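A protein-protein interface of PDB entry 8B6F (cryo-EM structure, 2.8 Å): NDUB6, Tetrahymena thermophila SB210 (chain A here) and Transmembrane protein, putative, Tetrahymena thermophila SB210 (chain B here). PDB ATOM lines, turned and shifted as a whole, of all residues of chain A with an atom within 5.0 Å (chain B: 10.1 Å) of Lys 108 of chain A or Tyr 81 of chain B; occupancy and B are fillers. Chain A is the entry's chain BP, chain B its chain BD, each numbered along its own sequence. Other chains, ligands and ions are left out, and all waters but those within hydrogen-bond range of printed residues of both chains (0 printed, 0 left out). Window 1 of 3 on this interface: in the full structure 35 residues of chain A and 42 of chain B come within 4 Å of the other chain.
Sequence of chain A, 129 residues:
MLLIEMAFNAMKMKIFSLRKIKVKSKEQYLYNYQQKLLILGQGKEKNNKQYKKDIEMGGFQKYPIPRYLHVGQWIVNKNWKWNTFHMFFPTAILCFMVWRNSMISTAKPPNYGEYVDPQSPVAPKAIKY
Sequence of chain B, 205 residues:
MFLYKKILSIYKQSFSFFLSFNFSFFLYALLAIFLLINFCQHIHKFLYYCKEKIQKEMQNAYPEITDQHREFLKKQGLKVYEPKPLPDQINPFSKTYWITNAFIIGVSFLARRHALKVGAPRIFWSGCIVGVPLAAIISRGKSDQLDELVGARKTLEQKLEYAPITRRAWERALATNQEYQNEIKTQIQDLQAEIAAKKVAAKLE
Of chain B, only Tyr 81 comes within 4 Å of Lys 108 of chain A. Of chain A, only Lys 108 (3.7 Å), Pro 110 (3.6 Å), Glu 114 (3.3 Å), Tyr 115 (2.7 Å), Val 116 (3.9 Å) and Val 122 (3.9 Å) come within 4 Å of Tyr 81 of chain B. No residue of chain B comes within 4 Å of Pro 109 of chain A. Pro 110 of chain A touches just one residue of chain B: Tyr 81 (3.6 Å). Of the printed residues of chain A, Gly 151 of chain B touches Val 122 (3.9 Å). Of the printed residues of chain A, Val 150 of chain B touches Ala 107. Printed residues of chain A within 4 Å of Leu 73 of chain B: Tyr 115. The nearest residue of chain B that does not touch Lys 108 of chain A is Lys 84 of chain B (4.6 Å).
Among the printed residues, pairs that only touch across the chains: Ala 107 of chain A with Val 150 of chain B, Lys 108 of chain A with Tyr 81 of chain B, Pro 110 of chain A with Tyr 81 of chain B, Glu 114 of chain A with Lys 79 of chain B, Glu 114 of chain A with Tyr 81 of chain B, Tyr 115 of chain A with Leu 73 of chain B, Tyr 115 of chain A with Leu 78 of chain B, Tyr 115 of chain A with Val 80 of chain B, Val 116 of chain A with Tyr 81 of chain B, Val 122 of chain A with Tyr 81 of chain B, Val 122 of chain A with Pro 83 of chain B and Val 122 of chain A with Gly 151 of chain B.
O of Lys 79 of chain B sits at hydrogen-bond distance from N of Tyr 115 of chain A (2.7 Å). O of Tyr 115 of chain A is in hydrogen-bond range of N of Tyr 81 of chain B.
Hydrophobic or aromatic side chains of chain B within 4 Å of the printed part of chain A: Leu 73, Leu 78, Val 80, Tyr 81, Pro 83 and Val 150. Of the 10 printed residues of chain A, 7 touch a printed residue of chain B. Hydrophobic or aromatic side chains of chain A within 4 Å of the printed part of chain B: Ala 107, Pro 110, Tyr 115, Val 116 and Val 122. Along chain A the printed residues that touch a printed residue of chain B span positions 107 to 122.
The backbone carbonyl oxygen (O) of Leu 73 of chain B sits at hydrogen-bond distance from the backbone NH (N) of Leu 78 of chain B (3.1 Å). The side-chain amide oxygen of Asn 111 of chain A sits at hydrogen-bond distance from the side-chain amino group of Lys 108 of chain A, 3.0 Å away. The side-chain carboxylate of Glu 114 of chain A lies within hydrogen-bond range of the side-chain amide nitrogen of Asn 111 of chain A (3.1 Å).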
ATOM      1  N   THR A 106     -15.821   7.285   6.900  1.00  0.00           N
ATOM      2  CA  THR A 106     -15.451   8.629   6.485  1.00  0.00           C
ATOM      3  C   THR A 106     -16.160   9.644   7.371  1.00  0.00           C
ATOM      4  O   THR A 106     -17.298   9.424   7.796  1.00  0.00           O
ATOM      5  CB  THR A 106     -15.817   8.873   5.017  1.00  0.00           C
ATOM      6  OG1 THR A 106     -15.098   7.955   4.185  1.00  0.00           O
ATOM      7  CG2 THR A 106     -15.481  10.298   4.594  1.00  0.00           C
ATOM      8  N   ALA A 107     -15.481  10.752   7.652  1.00  0.00           N
ATOM      9  CA  ALA A 107     -16.017  11.821   8.481  1.00  0.00           C
ATOM     10  C   ALA A 107     -15.966  13.136   7.718  1.00  0.00           C
ATOM     11  O   ALA A 107     -14.986  13.425   7.025  1.00  0.00           O
ATOM     12  CB  ALA A 107     -15.238  11.948   9.791  1.00  0.00           C
ATOM     13  N   LYS A 108     -17.032  13.925   7.844  1.00  0.00           N
ATOM     14  CA  LYS A 108     -17.149  15.213   7.187  1.00  0.00           C
ATOM     15  C   LYS A 108     -17.715  16.213   8.186  1.00  0.00           C
ATOM     16  O   LYS A 108     -18.566  15.846   9.009  1.00  0.00           O
ATOM     17  CB  LYS A 108     -18.063  15.130   5.955  1.00  0.00           C
ATOM     18  CG  LYS A 108     -18.151  16.414   5.146  1.00  0.00           C
ATOM     19  CD  LYS A 108     -19.305  16.380   4.158  1.00  0.00           C
ATOM     20  CE  LYS A 108     -20.646  16.510   4.866  1.00  0.00           C
ATOM     21  NZ  LYS A 108     -21.767  16.713   3.908  1.00  0.00           N
ATOM     22  N   PRO A 109     -17.272  17.468   8.150  1.00  0.00           N
ATOM     23  CA  PRO A 109     -17.846  18.477   9.044  1.00  0.00           C
ATOM     24  C   PRO A 109     -19.241  18.870   8.592  1.00  0.00           C
ATOM     25  O   PRO A 109     -19.629  18.605   7.446  1.00  0.00           O
ATOM     26  CB  PRO A 109     -16.865  19.652   8.925  1.00  0.00           C
ATOM     27  CG  PRO A 109     -16.261  19.493   7.588  1.00  0.00           C
ATOM     28  CD  PRO A 109     -16.156  18.016   7.360  1.00  0.00           C
ATOM     29  N   PRO A 110     -20.027  19.501   9.464  1.00  0.00           N
ATOM     30  CA  PRO A 110     -21.378  19.914   9.070  1.00  0.00           C
ATOM     31  C   PRO A 110     -21.361  20.826   7.851  1.00  0.00           C
ATOM     32  O   PRO A 110     -20.334  21.394   7.477  1.00  0.00           O
ATOM     33  CB  PRO A 110     -21.902  20.651  10.309  1.00  0.00           C
ATOM     34  CG  PRO A 110     -21.104  20.114  11.435  1.00  0.00           C
ATOM     35  CD  PRO A 110     -19.747  19.811  10.876  1.00  0.00           C
ATOM     36  N   ASN A 111     -22.529  20.959   7.228  1.00  0.00           N
ATOM     37  CA  ASN A 111     -22.670  21.770   6.026  1.00  0.00           C
ATOM     38  C   ASN A 111     -22.784  23.245   6.408  1.00  0.00           C
ATOM     39  O   ASN A 111     -22.576  23.636   7.560  1.00  0.00           O
ATOM     40  CB  ASN A 111     -23.872  21.299   5.208  1.00  0.00           C
ATOM     41  CG  ASN A 111     -23.654  19.938   4.583  1.00  0.00           C
ATOM     42  OD1 ASN A 111     -22.529  19.563   4.262  1.00  0.00           O
ATOM     43  ND2 ASN A 111     -24.736  19.191   4.402  1.00  0.00           N
ATOM     44  N   GLU A 114     -25.804  24.102   8.978  1.00  0.00           N
ATOM     45  CA  GLU A 114     -25.966  23.138  10.057  1.00  0.00           C
ATOM     46  C   GLU A 114     -25.063  23.487  11.232  1.00  0.00           C
ATOM     47  O   GLU A 114     -23.916  23.903  11.047  1.00  0.00           O
ATOM     48  CB  GLU A 114     -25.649  21.722   9.566  1.00  0.00           C
ATOM     49  CG  GLU A 114     -26.508  21.274   8.395  1.00  0.00           C
ATOM     50  CD  GLU A 114     -26.062  19.947   7.818  1.00  0.00           C
ATOM     51  OE1 GLU A 114     -25.095  19.364   8.348  1.00  0.00           O
ATOM     52  OE2 GLU A 114     -26.676  19.489   6.833  1.00  0.00           O
ATOM     53  N   TYR A 115     -25.592  23.311  12.440  1.00  0.00           N
ATOM     54  CA  TYR A 115     -24.834  23.486  13.669  1.00  0.00           C
ATOM     55  C   TYR A 115     -24.979  22.233  14.520  1.00  0.00           C
ATOM     56  O   TYR A 115     -26.018  21.567  14.499  1.00  0.00           O
ATOM     57  CB  TYR A 115     -25.310  24.712  14.463  1.00  0.00           C
ATOM     58  CG  TYR A 115     -26.571  24.478  15.263  1.00  0.00           C
ATOM     59  CD1 TYR A 115     -27.823  24.597  14.677  1.00  0.00           C
ATOM     60  CD2 TYR A 115     -26.507  24.146  16.610  1.00  0.00           C
ATOM     61  CE1 TYR A 115     -28.976  24.386  15.408  1.00  0.00           C
ATOM     62  CE2 TYR A 115     -27.654  23.932  17.349  1.00  0.00           C
ATOM     63  CZ  TYR A 115     -28.885  24.054  16.742  1.00  0.00           C
ATOM     64  OH  TYR A 115     -30.028  23.843  17.473  1.00  0.00           O
ATOM     65  N   VAL A 116     -23.929  21.914  15.268  1.00  0.00           N
ATOM     66  CA  VAL A 116     -23.896  20.709  16.086  1.00  0.00           C
ATOM     67  C   VAL A 116     -24.487  21.033  17.450  1.00  0.00           C
ATOM     68  O   VAL A 116     -23.973  21.894  18.171  1.00  0.00           O
ATOM     69  CB  VAL A 116     -22.464  20.167  16.219  1.00  0.00           C
ATOM     70  CG1 VAL A 116     -22.426  18.959  17.146  1.00  0.00           C
ATOM     71  CG2 VAL A 116     -21.907  19.809  14.853  1.00  0.00           C
ATOM     72  N   VAL A 122     -24.187  12.798  18.885  1.00  0.00           N
ATOM     73  CA  VAL A 122     -23.031  12.939  18.003  1.00  0.00           C
ATOM     74  C   VAL A 122     -22.001  13.887  18.595  1.00  0.00           C
ATOM     75  O   VAL A 122     -20.806  13.780  18.296  1.00  0.00           O
ATOM     76  CB  VAL A 122     -23.490  13.401  16.611  1.00  0.00           C
ATOM     77  CG1 VAL A 122     -22.299  13.626  15.687  1.00  0.00           C
ATOM     78  CG2 VAL A 122     -24.420  12.379  16.031  1.00  0.00           C
ATOM     79  N   TYR B  62     -19.389  19.438  25.955  1.00  0.00           N
ATOM     80  CA  TYR B  62     -19.617  20.846  25.684  1.00  0.00           C
ATOM     81  C   TYR B  62     -20.572  21.441  26.716  1.00  0.00           C
ATOM     82  O   TYR B  62     -21.379  20.725  27.316  1.00  0.00           O
ATOM     83  CB  TYR B  62     -20.200  21.037  24.286  1.00  0.00           C
ATOM     84  CG  TYR B  62     -19.251  20.722  23.151  1.00  0.00           C
ATOM     85  CD1 TYR B  62     -17.910  20.439  23.386  1.00  0.00           C
ATOM     86  CD2 TYR B  62     -19.699  20.720  21.838  1.00  0.00           C
ATOM     87  CE1 TYR B  62     -17.048  20.158  22.347  1.00  0.00           C
ATOM     88  CE2 TYR B  62     -18.844  20.440  20.792  1.00  0.00           C
ATOM     89  CZ  TYR B  62     -17.521  20.157  21.055  1.00  0.00           C
ATOM     90  OH  TYR B  62     -16.664  19.876  20.017  1.00  0.00           O
ATOM     91  N   ARG B  70     -32.406  26.925  21.391  1.00  0.00           N
ATOM     92  CA  ARG B  70     -32.574  26.054  20.233  1.00  0.00           C
ATOM     93  C   ARG B  70     -33.705  26.546  19.339  1.00  0.00           C
ATOM     94  O   ARG B  70     -33.566  26.583  18.112  1.00  0.00           O
ATOM     95  CB  ARG B  70     -32.846  24.620  20.683  1.00  0.00           C
ATOM     96  CG  ARG B  70     -31.658  23.927  21.320  1.00  0.00           C
ATOM     97  CD  ARG B  70     -31.976  22.469  21.605  1.00  0.00           C
ATOM     98  NE  ARG B  70     -30.823  21.759  22.143  1.00  0.00           N
ATOM     99  CZ  ARG B  70     -30.499  21.711  23.427  1.00  0.00           C
ATOM    100  NH1 ARG B  70     -31.222  22.329  24.347  1.00  0.00           N
ATOM    101  NH2 ARG B  70     -29.419  21.032  23.798  1.00  0.00           N
ATOM    102  N   LEU B  73     -32.573  29.598  17.422  1.00  0.00           N
ATOM    103  CA  LEU B  73     -31.758  29.228  16.269  1.00  0.00           C
ATOM    104  C   LEU B  73     -32.621  28.663  15.150  1.00  0.00           C
ATOM    105  O   LEU B  73     -32.398  28.960  13.971  1.00  0.00           O
ATOM    106  CB  LEU B  73     -30.688  28.219  16.682  1.00  0.00           C
ATOM    107  CG  LEU B  73     -29.655  28.705  17.702  1.00  0.00           C
ATOM    108  CD1 LEU B  73     -28.719  27.570  18.073  1.00  0.00           C
ATOM    109  CD2 LEU B  73     -28.870  29.899  17.182  1.00  0.00           C
ATOM    110  N   GLY B  77     -33.093  30.066  11.314  1.00  0.00           N
ATOM    111  CA  GLY B  77     -32.966  29.267  10.114  1.00  0.00           C
ATOM    112  C   GLY B  77     -31.855  28.241  10.127  1.00  0.00           C
ATOM    113  O   GLY B  77     -31.623  27.597   9.099  1.00  0.00           O
ATOM    114  N   LEU B  78     -31.157  28.071  11.246  1.00  0.00           N
ATOM    115  CA  LEU B  78     -30.132  27.045  11.328  1.00  0.00           C
ATOM    116  C   LEU B  78     -30.773  25.668  11.455  1.00  0.00           C
ATOM    117  O   LEU B  78     -31.961  25.528  11.753  1.00  0.00           O
ATOM    118  CB  LEU B  78     -29.210  27.300  12.517  1.00  0.00           C
ATOM    119  CG  LEU B  78     -28.628  28.709  12.622  1.00  0.00           C
ATOM    120  CD1 LEU B  78     -27.597  28.751  13.728  1.00  0.00           C
ATOM    121  CD2 LEU B  78     -28.028  29.166  11.303  1.00  0.00           C
ATOM    122  N   LYS B  79     -29.962  24.640  11.225  1.00  0.00           N
ATOM    123  CA  LYS B  79     -30.409  23.260  11.306  1.00  0.00           C
ATOM    124  C   LYS B  79     -29.462  22.473  12.199  1.00  0.00           C
ATOM    125  O   LYS B  79     -28.268  22.770  12.282  1.00  0.00           O
ATOM    126  CB  LYS B  79     -30.487  22.621   9.917  1.00  0.00           C
ATOM    127  CG  LYS B  79     -31.485  23.308   8.999  1.00  0.00           C
ATOM    128  CD  LYS B  79     -31.525  22.657   7.630  1.00  0.00           C
ATOM    129  CE  LYS B  79     -32.550  23.336   6.733  1.00  0.00           C
ATOM    130  NZ  LYS B  79     -32.602  22.716   5.379  1.00  0.00           N
ATOM    131  N   VAL B  80     -30.013  21.472  12.877  1.00  0.00           N
ATOM    132  CA  VAL B  80     -29.236  20.649  13.796  1.00  0.00           C
ATOM    133  C   VAL B  80     -28.523  19.571  12.991  1.00  0.00           C
ATOM    134  O   VAL B  80     -29.158  18.813  12.252  1.00  0.00           O
ATOM    135  CB  VAL B  80     -30.133  20.028  14.876  1.00  0.00           C
ATOM    136  CG1 VAL B  80     -29.292  19.278  15.898  1.00  0.00           C
ATOM    137  CG2 VAL B  80     -30.967  21.099  15.556  1.00  0.00           C
ATOM    138  N   TYR B  81     -27.203  19.501  13.131  1.00  0.00           N
ATOM    139  CA  TYR B  81     -26.442  18.478  12.430  1.00  0.00           C
ATOM    140  C   TYR B  81     -26.917  17.093  12.844  1.00  0.00           C
ATOM    141  O   TYR B  81     -27.045  16.796  14.035  1.00  0.00           O
ATOM    142  CB  TYR B  81     -24.952  18.637  12.728  1.00  0.00           C
ATOM    143  CG  TYR B  81     -24.094  17.552  12.130  1.00  0.00           C
ATOM    144  CD1 TYR B  81     -23.755  17.570  10.784  1.00  0.00           C
ATOM    145  CD2 TYR B  81     -23.614  16.512  12.913  1.00  0.00           C
ATOM    146  CE1 TYR B  81     -22.967  16.579  10.236  1.00  0.00           C
ATOM    147  CE2 TYR B  81     -22.826  15.518  12.375  1.00  0.00           C
ATOM    148  CZ  TYR B  81     -22.505  15.557  11.035  1.00  0.00           C
ATOM    149  OH  TYR B  81     -21.717  14.567  10.495  1.00  0.00           O
ATOM    150  N   GLU B  82     -27.174  16.245  11.851  1.00  0.00           N
ATOM    151  CA  GLU B  82     -27.672  14.901  12.102  1.00  0.00           C
ATOM    152  C   GLU B  82     -26.985  13.923  11.156  1.00  0.00           C
ATOM    153  O   GLU B  82     -27.026  14.114   9.935  1.00  0.00           O
ATOM    154  CB  GLU B  82     -29.189  14.849  11.915  1.00  0.00           C
ATOM    155  CG  GLU B  82     -29.841  13.584  12.446  1.00  0.00           C
ATOM    156  CD  GLU B  82     -29.841  13.520  13.960  1.00  0.00           C
ATOM    157  OE1 GLU B  82     -29.365  14.483  14.598  1.00  0.00           O
ATOM    158  OE2 GLU B  82     -30.323  12.511  14.515  1.00  0.00           O
ATOM    159  N   PRO B  83     -26.342  12.874  11.668  1.00  0.00           N
ATOM    160  CA  PRO B  83     -25.702  11.900  10.778  1.00  0.00           C
ATOM    161  C   PRO B  83     -26.727  11.230   9.877  1.00  0.00           C
ATOM    162  O   PRO B  83     -27.855  10.950  10.290  1.00  0.00           O
ATOM    163  CB  PRO B  83     -25.049  10.908  11.745  1.00  0.00           C
ATOM    164  CG  PRO B  83     -25.835  11.031  12.995  1.00  0.00           C
ATOM    165  CD  PRO B  83     -26.251  12.468  13.076  1.00  0.00           C
ATOM    166  N   LYS B  84     -26.325  10.972   8.648  1.00  0.00           N
ATOM    167  CA  LYS B  84     -27.246  10.414   7.675  1.00  0.00           C
ATOM    168  C   LYS B  84     -26.966   8.933   7.449  1.00  0.00           C
ATOM    169  O   LYS B  84     -25.813   8.496   7.497  1.00  0.00           O
ATOM    170  CB  LYS B  84     -27.134  11.163   6.345  1.00  0.00           C
ATOM    171  CG  LYS B  84     -27.605  12.606   6.431  1.00  0.00           C
ATOM    172  CD  LYS B  84     -27.420  13.347   5.117  1.00  0.00           C
ATOM    173  CE  LYS B  84     -25.956  13.667   4.858  1.00  0.00           C
ATOM    174  NZ  LYS B  84     -25.788  14.533   3.658  1.00  0.00           N
ATOM    175  N   PRO B  85     -28.000   8.131   7.200  1.00  0.00           N
ATOM    176  CA  PRO B  85     -27.776   6.701   6.975  1.00  0.00           C
ATOM    177  C   PRO B  85     -27.004   6.451   5.691  1.00  0.00           C
ATOM    178  O   PRO B  85     -27.057   7.235   4.740  1.00  0.00           O
ATOM    179  CB  PRO B  85     -29.195   6.128   6.894  1.00  0.00           C
ATOM    180  CG  PRO B  85     -30.033   7.269   6.449  1.00  0.00           C
ATOM    181  CD  PRO B  85     -29.422   8.493   7.064  1.00  0.00           C
ATOM    182  N   LEU B 149     -16.095   5.897  15.526  1.00  0.00           N
ATOM    183  CA  LEU B 149     -15.407   6.959  14.815  1.00  0.00           C
ATOM    184  C   LEU B 149     -16.291   8.202  14.821  1.00  0.00           C
ATOM    185  O   LEU B 149     -17.375   8.225  15.410  1.00  0.00           O
ATOM    186  CB  LEU B 149     -15.071   6.514  13.393  1.00  0.00           C
ATOM    187  CG  LEU B 149     -13.998   7.309  12.642  1.00  0.00           C
ATOM    188  CD1 LEU B 149     -12.879   6.386  12.192  1.00  0.00           C
ATOM    189  CD2 LEU B 149     -14.591   8.043  11.450  1.00  0.00           C
ATOM    190  N   VAL B 150     -15.830   9.259  14.165  1.00  0.00           N
ATOM    191  CA  VAL B 150     -16.633  10.469  14.059  1.00  0.00           C
ATOM    192  C   VAL B 150     -17.886  10.129  13.266  1.00  0.00           C
ATOM    193  O   VAL B 150     -17.820   9.835  12.069  1.00  0.00           O
ATOM    194  CB  VAL B 150     -15.840  11.617  13.416  1.00  0.00           C
ATOM    195  CG1 VAL B 150     -16.658  12.897  13.398  1.00  0.00           C
ATOM    196  CG2 VAL B 150     -14.549  11.815  14.174  1.00  0.00           C
ATOM    197  N   GLY B 151     -19.032  10.167  13.932  1.00  0.00           N
ATOM    198  CA  GLY B 151     -20.277   9.761  13.311  1.00  0.00           C
ATOM    199  C   GLY B 151     -21.308   9.434  14.376  1.00  0.00           C
ATOM    200  O   GLY B 151     -21.181   9.842  15.529  1.00  0.00           O
ATOM    201  N   ALA B 152     -22.325   8.687  13.960  1.00  0.00           N
ATOM    202  CA  ALA B 152     -23.403   8.329  14.870  1.00  0.00           C
ATOM    203  C   ALA B 152     -22.880   7.468  16.011  1.00  0.00           C
ATOM    204  O   ALA B 152     -22.108   6.529  15.796  1.00  0.00           O
ATOM    205  CB  ALA B 152     -24.503   7.591  14.110  1.00  0.00           C
ATOM    206  N   ARG B 153     -23.303   7.794  17.228  1.00  0.00           N
ATOM    207  CA  ARG B 153     -22.925   7.018  18.399  1.00  0.00           C
ATOM    208  C   ARG B 153     -23.704   5.711  18.446  1.00  0.00           C
ATOM    209  O   ARG B 153     -24.872   5.643  18.056  1.00  0.00           O
ATOM    210  CB  ARG B 153     -23.185   7.809  19.683  1.00  0.00           C
ATOM    211  CG  ARG B 153     -22.332   9.053  19.848  1.00  0.00           C
ATOM    212  CD  ARG B 153     -20.854   8.711  19.906  1.00  0.00           C
ATOM    213  NE  ARG B 153     -20.036   9.884  20.187  1.00  0.00           N
ATOM    214  CZ  ARG B 153     -19.693  10.295  21.400  1.00  0.00           C
ATOM    215  NH1 ARG B 153     -20.088   9.653  22.486  1.00  0.00           N
ATOM    216  NH2 ARG B 153     -18.933  11.378  21.525  1.00  0.00           N
